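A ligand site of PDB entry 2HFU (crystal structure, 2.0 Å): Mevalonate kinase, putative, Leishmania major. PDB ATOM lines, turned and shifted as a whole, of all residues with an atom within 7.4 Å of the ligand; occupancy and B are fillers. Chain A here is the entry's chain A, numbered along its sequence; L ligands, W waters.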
ATOM      1  N   LYS A  21      19.238  -7.780   8.997  1.00  0.00           N
ATOM      2  CA  LYS A  21      18.307  -7.495   7.911  1.00  0.00           C
ATOM      3  C   LYS A  21      17.684  -8.769   7.363  1.00  0.00           C
ATOM      4  O   LYS A  21      18.378  -9.770   7.164  1.00  0.00           O
ATOM      5  CB  LYS A  21      19.050  -6.774   6.773  1.00  0.00           C
ATOM      6  CG  LYS A  21      18.247  -6.653   5.474  1.00  0.00           C
ATOM      7  CD  LYS A  21      19.022  -7.113   4.239  1.00  0.00           C
ATOM      8  CE  LYS A  21      19.305  -8.620   4.254  1.00  0.00           C
ATOM      9  NZ  LYS A  21      19.660  -9.155   2.913  1.00  0.00           N
ATOM     10  N   ILE A  23      14.858  -9.595   4.035  1.00  0.00           N
ATOM     11  CA  ILE A  23      13.950  -9.079   3.020  1.00  0.00           C
ATOM     12  C   ILE A  23      12.609  -9.775   3.174  1.00  0.00           C
ATOM     13  O   ILE A  23      12.509 -10.995   3.056  1.00  0.00           O
ATOM     14  CB  ILE A  23      14.538  -9.228   1.594  1.00  0.00           C
ATOM     15  CG1 ILE A  23      15.757  -8.314   1.433  1.00  0.00           C
ATOM     16  CG2 ILE A  23      13.469  -8.879   0.551  1.00  0.00           C
ATOM     17  CD1 ILE A  23      16.530  -8.497   0.127  1.00  0.00           C
ATOM     18  N   GLY A  26      10.032  -8.875  -2.082  1.00  0.00           N
ATOM     19  CA  GLY A  26      10.447  -8.204  -3.298  1.00  0.00           C
ATOM     20  C   GLY A  26      11.878  -8.442  -3.770  1.00  0.00           C
ATOM     21  O   GLY A  26      12.327  -7.814  -4.701  1.00  0.00           O
ATOM     22  N   GLU A  27      12.585  -9.375  -3.145  1.00  0.00           N
ATOM     23  CA  GLU A  27      13.881  -9.786  -3.670  1.00  0.00           C
ATOM     24  C   GLU A  27      13.739 -10.146  -5.147  1.00  0.00           C
ATOM     25  O   GLU A  27      12.706 -10.686  -5.573  1.00  0.00           O
ATOM     26  CB  GLU A  27      14.482 -10.950  -2.883  1.00  0.00           C
ATOM     27  CG  GLU A  27      13.603 -12.190  -2.766  1.00  0.00           C
ATOM     28  CD  GLU A  27      12.746 -12.158  -1.522  1.00  0.00           C
ATOM     29  OE1 GLU A  27      13.300 -12.298  -0.415  1.00  0.00           O
ATOM     30  OE2 GLU A  27      11.515 -11.981  -1.647  1.00  0.00           O
ATOM     31  N   HIS A  28      14.767  -9.807  -5.916  1.00  0.00           N
ATOM     32  CA  HIS A  28      14.842 -10.034  -7.370  1.00  0.00           C
ATOM     33  C   HIS A  28      13.933  -9.148  -8.221  1.00  0.00           C
ATOM     34  O   HIS A  28      14.386  -8.588  -9.225  1.00  0.00           O
ATOM     35  CB  HIS A  28      14.654 -11.514  -7.720  1.00  0.00           C
ATOM     36  CG  HIS A  28      15.793 -12.371  -7.278  1.00  0.00           C
ATOM     37  ND1 HIS A  28      16.992 -12.424  -7.946  1.00  0.00           N
ATOM     38  CD2 HIS A  28      15.923 -13.204  -6.213  1.00  0.00           C
ATOM     39  CE1 HIS A  28      17.813 -13.257  -7.324  1.00  0.00           C
ATOM     40  NE2 HIS A  28      17.188 -13.740  -6.265  1.00  0.00           N
ATOM     41  N   PHE A  29      12.675  -9.010  -7.823  1.00  0.00           N
ATOM     42  CA  PHE A  29      11.734  -8.160  -8.558  1.00  0.00           C
ATOM     43  C   PHE A  29      12.069  -6.674  -8.401  1.00  0.00           C
ATOM     44  O   PHE A  29      11.797  -5.879  -9.307  1.00  0.00           O
ATOM     45  CB  PHE A  29      10.288  -8.437  -8.122  1.00  0.00           C
ATOM     46  CG  PHE A  29       9.820  -9.827  -8.453  1.00  0.00           C
ATOM     47  CD1 PHE A  29       9.538 -10.730  -7.439  1.00  0.00           C
ATOM     48  CD2 PHE A  29       9.668 -10.233  -9.782  1.00  0.00           C
ATOM     49  CE1 PHE A  29       9.118 -12.030  -7.741  1.00  0.00           C
ATOM     50  CE2 PHE A  29       9.247 -11.520 -10.093  1.00  0.00           C
ATOM     51  CZ  PHE A  29       8.967 -12.422  -9.064  1.00  0.00           C
ATOM     52  N   VAL A  30      12.676  -6.322  -7.269  1.00  0.00           N
ATOM     53  CA  VAL A  30      13.106  -4.944  -7.003  1.00  0.00           C
ATOM     54  C   VAL A  30      14.143  -4.462  -8.027  1.00  0.00           C
ATOM     55  O   VAL A  30      14.205  -3.272  -8.338  1.00  0.00           O
ATOM     56  CB  VAL A  30      13.646  -4.799  -5.551  1.00  0.00           C
ATOM     57  CG1 VAL A  30      14.906  -5.644  -5.327  1.00  0.00           C
ATOM     58  CG2 VAL A  30      13.878  -3.326  -5.178  1.00  0.00           C
ATOM     59  N   VAL A  31      14.947  -5.396  -8.541  1.00  0.00           N
ATOM     60  CA  VAL A  31      15.961  -5.110  -9.561  1.00  0.00           C
ATOM     61  C   VAL A  31      15.292  -4.562 -10.828  1.00  0.00           C
ATOM     62  O   VAL A  31      15.895  -3.773 -11.564  1.00  0.00           O
ATOM     63  CB  VAL A  31      16.806  -6.368  -9.876  1.00  0.00           C
ATOM     64  CG1 VAL A  31      17.857  -6.092 -10.965  1.00  0.00           C
ATOM     65  CG2 VAL A  31      17.481  -6.900  -8.612  1.00  0.00           C
ATOM     66  N   ALA A  36      10.140  -3.111  -2.762  1.00  0.00           N
ATOM     67  CA  ALA A  36      10.537  -4.148  -1.834  1.00  0.00           C
ATOM     68  C   ALA A  36      10.328  -3.710  -0.385  1.00  0.00           C
ATOM     69  O   ALA A  36      10.402  -2.523  -0.074  1.00  0.00           O
ATOM     70  CB  ALA A  36      11.984  -4.560  -2.073  1.00  0.00           C
ATOM     71  N   GLY A 111      22.829 -13.885   3.860  1.00  0.00           N
ATOM     72  CA  GLY A 111      21.437 -13.443   3.737  1.00  0.00           C
ATOM     73  C   GLY A 111      20.908 -12.539   4.844  1.00  0.00           C
ATOM     74  O   GLY A 111      19.826 -11.961   4.702  1.00  0.00           O
ATOM     75  N   THR A 153      27.636  -6.297  -5.875  1.00  0.00           N
ATOM     76  CA  THR A 153      27.719  -4.939  -5.329  1.00  0.00           C
ATOM     77  C   THR A 153      26.572  -4.652  -4.335  1.00  0.00           C
ATOM     78  O   THR A 153      25.494  -5.239  -4.450  1.00  0.00           O
ATOM     79  CB  THR A 153      27.711  -3.926  -6.518  1.00  0.00           C
ATOM     80  OG1 THR A 153      29.054  -3.694  -6.972  1.00  0.00           O
ATOM     81  CG2 THR A 153      27.231  -2.521  -6.124  1.00  0.00           C
ATOM     82  N   PRO A 154      26.818  -3.781  -3.350  1.00  0.00           N
ATOM     83  CA  PRO A 154      25.771  -3.353  -2.425  1.00  0.00           C
ATOM     84  C   PRO A 154      24.683  -2.506  -3.089  1.00  0.00           C
ATOM     85  O   PRO A 154      24.977  -1.528  -3.782  1.00  0.00           O
ATOM     86  CB  PRO A 154      26.520  -2.508  -1.388  1.00  0.00           C
ATOM     87  CG  PRO A 154      27.965  -2.814  -1.585  1.00  0.00           C
ATOM     88  CD  PRO A 154      28.119  -3.156  -3.027  1.00  0.00           C
ATOM     89  N   SER A 155      23.424  -2.895  -2.871  1.00  0.00           N
ATOM     90  CA  SER A 155      22.268  -2.133  -3.340  1.00  0.00           C
ATOM     91  C   SER A 155      22.009  -0.925  -2.453  1.00  0.00           C
ATOM     92  O   SER A 155      21.424   0.063  -2.885  1.00  0.00           O
ATOM     93  CB  SER A 155      21.030  -3.021  -3.365  1.00  0.00           C
ATOM     94  OG  SER A 155      20.637  -3.378  -2.055  1.00  0.00           O
ATOM     95  N   GLY A 156      22.451  -1.023  -1.197  1.00  0.00           N
ATOM     96  CA  GLY A 156      22.184   0.010  -0.202  1.00  0.00           C
ATOM     97  C   GLY A 156      21.173  -0.443   0.838  1.00  0.00           C
ATOM     98  O   GLY A 156      21.092   0.147   1.921  1.00  0.00           O
ATOM     99  N   ALA A 157      20.414  -1.487   0.514  1.00  0.00           N
ATOM    100  CA  ALA A 157      19.372  -2.018   1.392  1.00  0.00           C
ATOM    101  C   ALA A 157      19.931  -2.556   2.709  1.00  0.00           C
ATOM    102  O   ALA A 157      19.358  -2.307   3.767  1.00  0.00           O
ATOM    103  CB  ALA A 157      18.574  -3.106   0.683  1.00  0.00           C
ATOM    104  N   ASP A 158      21.040  -3.281   2.623  1.00  0.00           N
ATOM    105  CA  ASP A 158      21.671  -3.876   3.798  1.00  0.00           C
ATOM    106  C   ASP A 158      22.134  -2.800   4.785  1.00  0.00           C
ATOM    107  O   ASP A 158      21.742  -2.829   5.947  1.00  0.00           O
ATOM    108  CB  ASP A 158      22.849  -4.778   3.407  1.00  0.00           C
ATOM    109  CG  ASP A 158      22.414  -6.032   2.659  1.00  0.00           C
ATOM    110  OD1 ASP A 158      21.233  -6.143   2.285  1.00  0.00           O
ATOM    111  OD2 ASP A 158      23.202  -6.969   2.406  1.00  0.00           O
ATOM    112  N   TYR A 170      11.945  -0.189  -0.135  1.00  0.00           N
ATOM    113  CA  TYR A 170      13.142  -0.132  -0.970  1.00  0.00           C
ATOM    114  C   TYR A 170      12.757  -0.294  -2.435  1.00  0.00           C
ATOM    115  O   TYR A 170      12.153  -1.294  -2.821  1.00  0.00           O
ATOM    116  CB  TYR A 170      14.141  -1.193  -0.484  1.00  0.00           C
ATOM    117  CG  TYR A 170      15.111  -1.790  -1.499  1.00  0.00           C
ATOM    118  CD1 TYR A 170      15.304  -3.176  -1.575  1.00  0.00           C
ATOM    119  CD2 TYR A 170      15.861  -0.973  -2.359  1.00  0.00           C
ATOM    120  CE1 TYR A 170      16.198  -3.731  -2.482  1.00  0.00           C
ATOM    121  CE2 TYR A 170      16.766  -1.533  -3.275  1.00  0.00           C
ATOM    122  CZ  TYR A 170      16.932  -2.912  -3.326  1.00  0.00           C
ATOM    123  OH  TYR A 170      17.804  -3.469  -4.223  1.00  0.00           O
ATOM    124  N   ARG A 172      14.075   0.983  -6.737  1.00  0.00           N
ATOM    125  CA  ARG A 172      14.978   1.651  -7.679  1.00  0.00           C
ATOM    126  C   ARG A 172      14.214   2.764  -8.374  1.00  0.00           C
ATOM    127  O   ARG A 172      13.278   2.511  -9.130  1.00  0.00           O
ATOM    128  CB  ARG A 172      15.516   0.644  -8.700  1.00  0.00           C
ATOM    129  CG  ARG A 172      16.116  -0.613  -8.099  1.00  0.00           C
ATOM    130  CD  ARG A 172      17.579  -0.494  -7.715  1.00  0.00           C
ATOM    131  NE  ARG A 172      18.124  -1.785  -7.296  1.00  0.00           N
ATOM    132  CZ  ARG A 172      19.405  -2.119  -7.367  1.00  0.00           C
ATOM    133  NH1 ARG A 172      20.297  -1.261  -7.842  1.00  0.00           N
ATOM    134  NH2 ARG A 172      19.794  -3.321  -6.955  1.00  0.00           N
ATOM    135  N   SER A 177      18.769   3.472  -5.835  1.00  0.00           N
ATOM    136  CA  SER A 177      18.019   2.928  -4.703  1.00  0.00           C
ATOM    137  C   SER A 177      17.457   4.017  -3.785  1.00  0.00           C
ATOM    138  O   SER A 177      18.208   4.848  -3.270  1.00  0.00           O
ATOM    139  CB  SER A 177      18.870   1.932  -3.908  1.00  0.00           C
ATOM    140  OG  SER A 177      19.092   0.745  -4.648  1.00  0.00           O
ATOM    141  N   THR A 201      24.799 -13.776  -5.393  1.00  0.00           N
ATOM    142  CA  THR A 201      23.786 -12.787  -5.757  1.00  0.00           C
ATOM    143  C   THR A 201      23.902 -12.385  -7.224  1.00  0.00           C
ATOM    144  O   THR A 201      22.912 -12.410  -7.955  1.00  0.00           O
ATOM    145  CB  THR A 201      23.889 -11.542  -4.839  1.00  0.00           C
ATOM    146  OG1 THR A 201      23.570 -11.921  -3.495  1.00  0.00           O
ATOM    147  CG2 THR A 201      22.803 -10.529  -5.187  1.00  0.00           C
ATOM    148  N   VAL A 204      22.686 -15.300  -9.685  1.00  0.00           N
ATOM    149  CA  VAL A 204      21.244 -15.532  -9.647  1.00  0.00           C
ATOM    150  C   VAL A 204      20.462 -14.372 -10.272  1.00  0.00           C
ATOM    151  O   VAL A 204      19.524 -14.602 -11.044  1.00  0.00           O
ATOM    152  CB  VAL A 204      20.727 -15.817  -8.196  1.00  0.00           C
ATOM    153  CG1 VAL A 204      19.287 -16.288  -8.218  1.00  0.00           C
ATOM    154  CG2 VAL A 204      21.597 -16.859  -7.507  1.00  0.00           C
ATOM    155  N   VAL A 205      20.864 -13.146  -9.961  1.00  0.00           N
ATOM    156  CA  VAL A 205      20.303 -11.946 -10.599  1.00  0.00           C
ATOM    157  C   VAL A 205      20.474 -11.988 -12.118  1.00  0.00           C
ATOM    158  O   VAL A 205      19.526 -11.731 -12.856  1.00  0.00           O
ATOM    159  CB  VAL A 205      20.902 -10.641  -9.979  1.00  0.00           C
ATOM    160  CG1 VAL A 205      20.636  -9.421 -10.854  1.00  0.00           C
ATOM    161  CG2 VAL A 205      20.367 -10.421  -8.566  1.00  0.00           C
ATOM    162  N   VAL A 208      18.173 -14.430 -13.645  1.00  0.00           N
ATOM    163  CA  VAL A 208      16.833 -13.833 -13.723  1.00  0.00           C
ATOM    164  C   VAL A 208      16.761 -12.851 -14.901  1.00  0.00           C
ATOM    165  O   VAL A 208      15.750 -12.830 -15.625  1.00  0.00           O
ATOM    166  CB  VAL A 208      16.417 -13.158 -12.384  1.00  0.00           C
ATOM    167  CG1 VAL A 208      15.094 -12.429 -12.533  1.00  0.00           C
ATOM    168  CG2 VAL A 208      16.309 -14.187 -11.270  1.00  0.00           C
ATOM    169  N   VAL A 261      14.427 -19.118  -8.275  1.00  0.00           N
ATOM    170  CA  VAL A 261      15.409 -18.694  -7.273  1.00  0.00           C
ATOM    171  C   VAL A 261      15.257 -19.455  -5.952  1.00  0.00           C
ATOM    172  O   VAL A 261      15.933 -19.162  -4.975  1.00  0.00           O
ATOM    173  CB  VAL A 261      15.418 -17.139  -7.047  1.00  0.00           C
ATOM    174  CG1 VAL A 261      15.738 -16.410  -8.332  1.00  0.00           C
ATOM    175  CG2 VAL A 261      14.093 -16.639  -6.453  1.00  0.00           C
ATOM    176  N   SER A 284      14.268 -15.655   1.598  1.00  0.00           N
ATOM    177  CA  SER A 284      14.574 -14.250   1.815  1.00  0.00           C
ATOM    178  C   SER A 284      15.917 -13.907   1.209  1.00  0.00           C
ATOM    179  O   SER A 284      16.946 -14.440   1.635  1.00  0.00           O
ATOM    180  CB  SER A 284      14.550 -13.905   3.310  1.00  0.00           C
ATOM    181  OG  SER A 284      14.897 -12.546   3.532  1.00  0.00           O
ATOM    182  N   GLY A 285      15.908 -13.030   0.209  1.00  0.00           N
ATOM    183  CA  GLY A 285      17.126 -12.530  -0.405  1.00  0.00           C
ATOM    184  C   GLY A 285      17.433 -13.181  -1.737  1.00  0.00           C
ATOM    185  O   GLY A 285      16.572 -13.310  -2.607  1.00  0.00           O
ATOM    186  N   THR A 286      18.689 -13.602  -1.883  1.00  0.00           N
ATOM    187  CA  THR A 286      19.195 -14.133  -3.146  1.00  0.00           C
ATOM    188  C   THR A 286      18.536 -15.458  -3.563  1.00  0.00           C
ATOM    189  O   THR A 286      18.338 -15.703  -4.755  1.00  0.00           O
ATOM    190  CB  THR A 286      20.729 -14.275  -3.074  1.00  0.00           C
ATOM    191  OG1 THR A 286      21.315 -12.968  -3.090  1.00  0.00           O
ATOM    192  CG2 THR A 286      21.290 -14.926  -4.342  1.00  0.00           C
ATOM    193  N   GLY A 287      18.199 -16.289  -2.589  1.00  0.00           N
ATOM    194  CA  GLY A 287      17.611 -17.604  -2.874  1.00  0.00           C
ATOM    195  C   GLY A 287      18.666 -18.600  -3.289  1.00  0.00           C
ATOM    196  O   GLY A 287      19.865 -18.317  -3.204  1.00  0.00           O
HETATM  197  C1  LIG L   1      19.619  -9.884  -2.748  1.00  0.00           C
HETATM  198  O1  LIG L   1      19.902  -9.633  -1.368  1.00  0.00           O
HETATM  199  C2  LIG L   1      18.360  -9.132  -3.158  1.00  0.00           C
HETATM  200  C3  LIG L   1      18.163  -8.974  -4.676  1.00  0.00           C
HETATM  201  O2  LIG L   1      16.872  -8.403  -4.895  1.00  0.00           O
HETATM  202  C4  LIG L   1      19.224  -8.073  -5.329  1.00  0.00           C
HETATM  203  C5  LIG L   1      19.101  -6.597  -4.991  1.00  0.00           C
HETATM  204  O3  LIG L   1      20.054  -5.845  -5.301  1.00  0.00           O
HETATM  205  O4  LIG L   1      18.064  -6.144  -4.456  1.00  0.00           O
HETATM  206  C6  LIG L   1      18.166 -10.333  -5.357  1.00  0.00           C
HETATM  207  O   HOH W   1      20.089  -7.066   0.157  1.00  0.00           O
HETATM  208  O   HOH W   2      22.895  -9.539  -1.631  1.00  0.00           O
HETATM  209  O   HOH W   3      19.347  -5.568  -1.884  1.00  0.00           O
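The guanidinium group (NH2) of Arg 172 sits at hydrogen-bond distance from the side-chain hydroxyl (OH) of Tyr 170.
The backbone carbonyl oxygen (O) of Tyr 170 sits at hydrogen-bond distance from the backbone NH (N) of Ala 36 (2.7 Å).
A ring nitrogen (NE2) of His 28 sits at hydrogen-bond distance from the backbone carbonyl oxygen of Thr 286 (2.7 Å).
The side-chain carboxylate of Glu 27 is in hydrogen-bond range of the backbone NH of Gly 285 (2.8 Å).
OG1 of Thr 201 lies within hydrogen-bond range of OG1 of Thr 286, 2.5 Å away.
N of Ala 157 is in hydrogen-bond range of OG of Ser 155 (3.2 Å).
The side-chain hydroxyl (OG) of Ser 177 lies within hydrogen-bond range of the backbone carbonyl oxygen (O) of Ser 155.
The backbone carbonyl oxygen (O) of Ile 23 is in hydrogen-bond range of the side-chain hydroxyl (OG) of Ser 284 (2.9 Å).
The side-chain hydroxyl (OH) of Tyr 170 lies within hydrogen-bond range of an oxygen (O4) of the ligand (2.7 Å).
N of His 28 sits at hydrogen-bond distance from O2 of the ligand (2.7 Å).
An oxygen (O3) of the ligand is in salt-bridge range of the guanidinium group of Arg 172, at 3.0 Å.
Residues that only touch the ligand: Val 30 (3.3 Å), Glu 27 (3.5 Å), Thr 286 (3.5 Å), Ser 155 (3.6 Å), Ile 23 (3.8 Å), Val 205 (3.9 Å) and Val 31 (3.9 Å).
Hydrophobic or aromatic side chains within 4 Å of the ligand: Ile 23, His 28, Val 30, Val 31, Tyr 170 and Val 205.
Within 4 Å of the ligand: Ile 23, Glu 27, His 28, Val 30, Val 31, Ser 155, Tyr 170, Arg 172, Val 205 and Thr 286.
Water W3 bridges the side-chain hydroxyl (OG) of Ser 155 (2.5 Å) and an oxygen (O4) of the ligand (2.9 Å).
Water W1 lies within hydrogen-bond range of the side-chain carboxylate (OD1) of Asp 158 (2.6 Å), an oxygen (O1) of the ligand (3.0 Å) and the side-chain amino group (NZ) of Lys 21 (3.5 Å).
Water W2 bridges an oxygen (O1) of the ligand (3.0 Å) and the side-chain hydroxyl of Thr 201 (3.1 Å).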
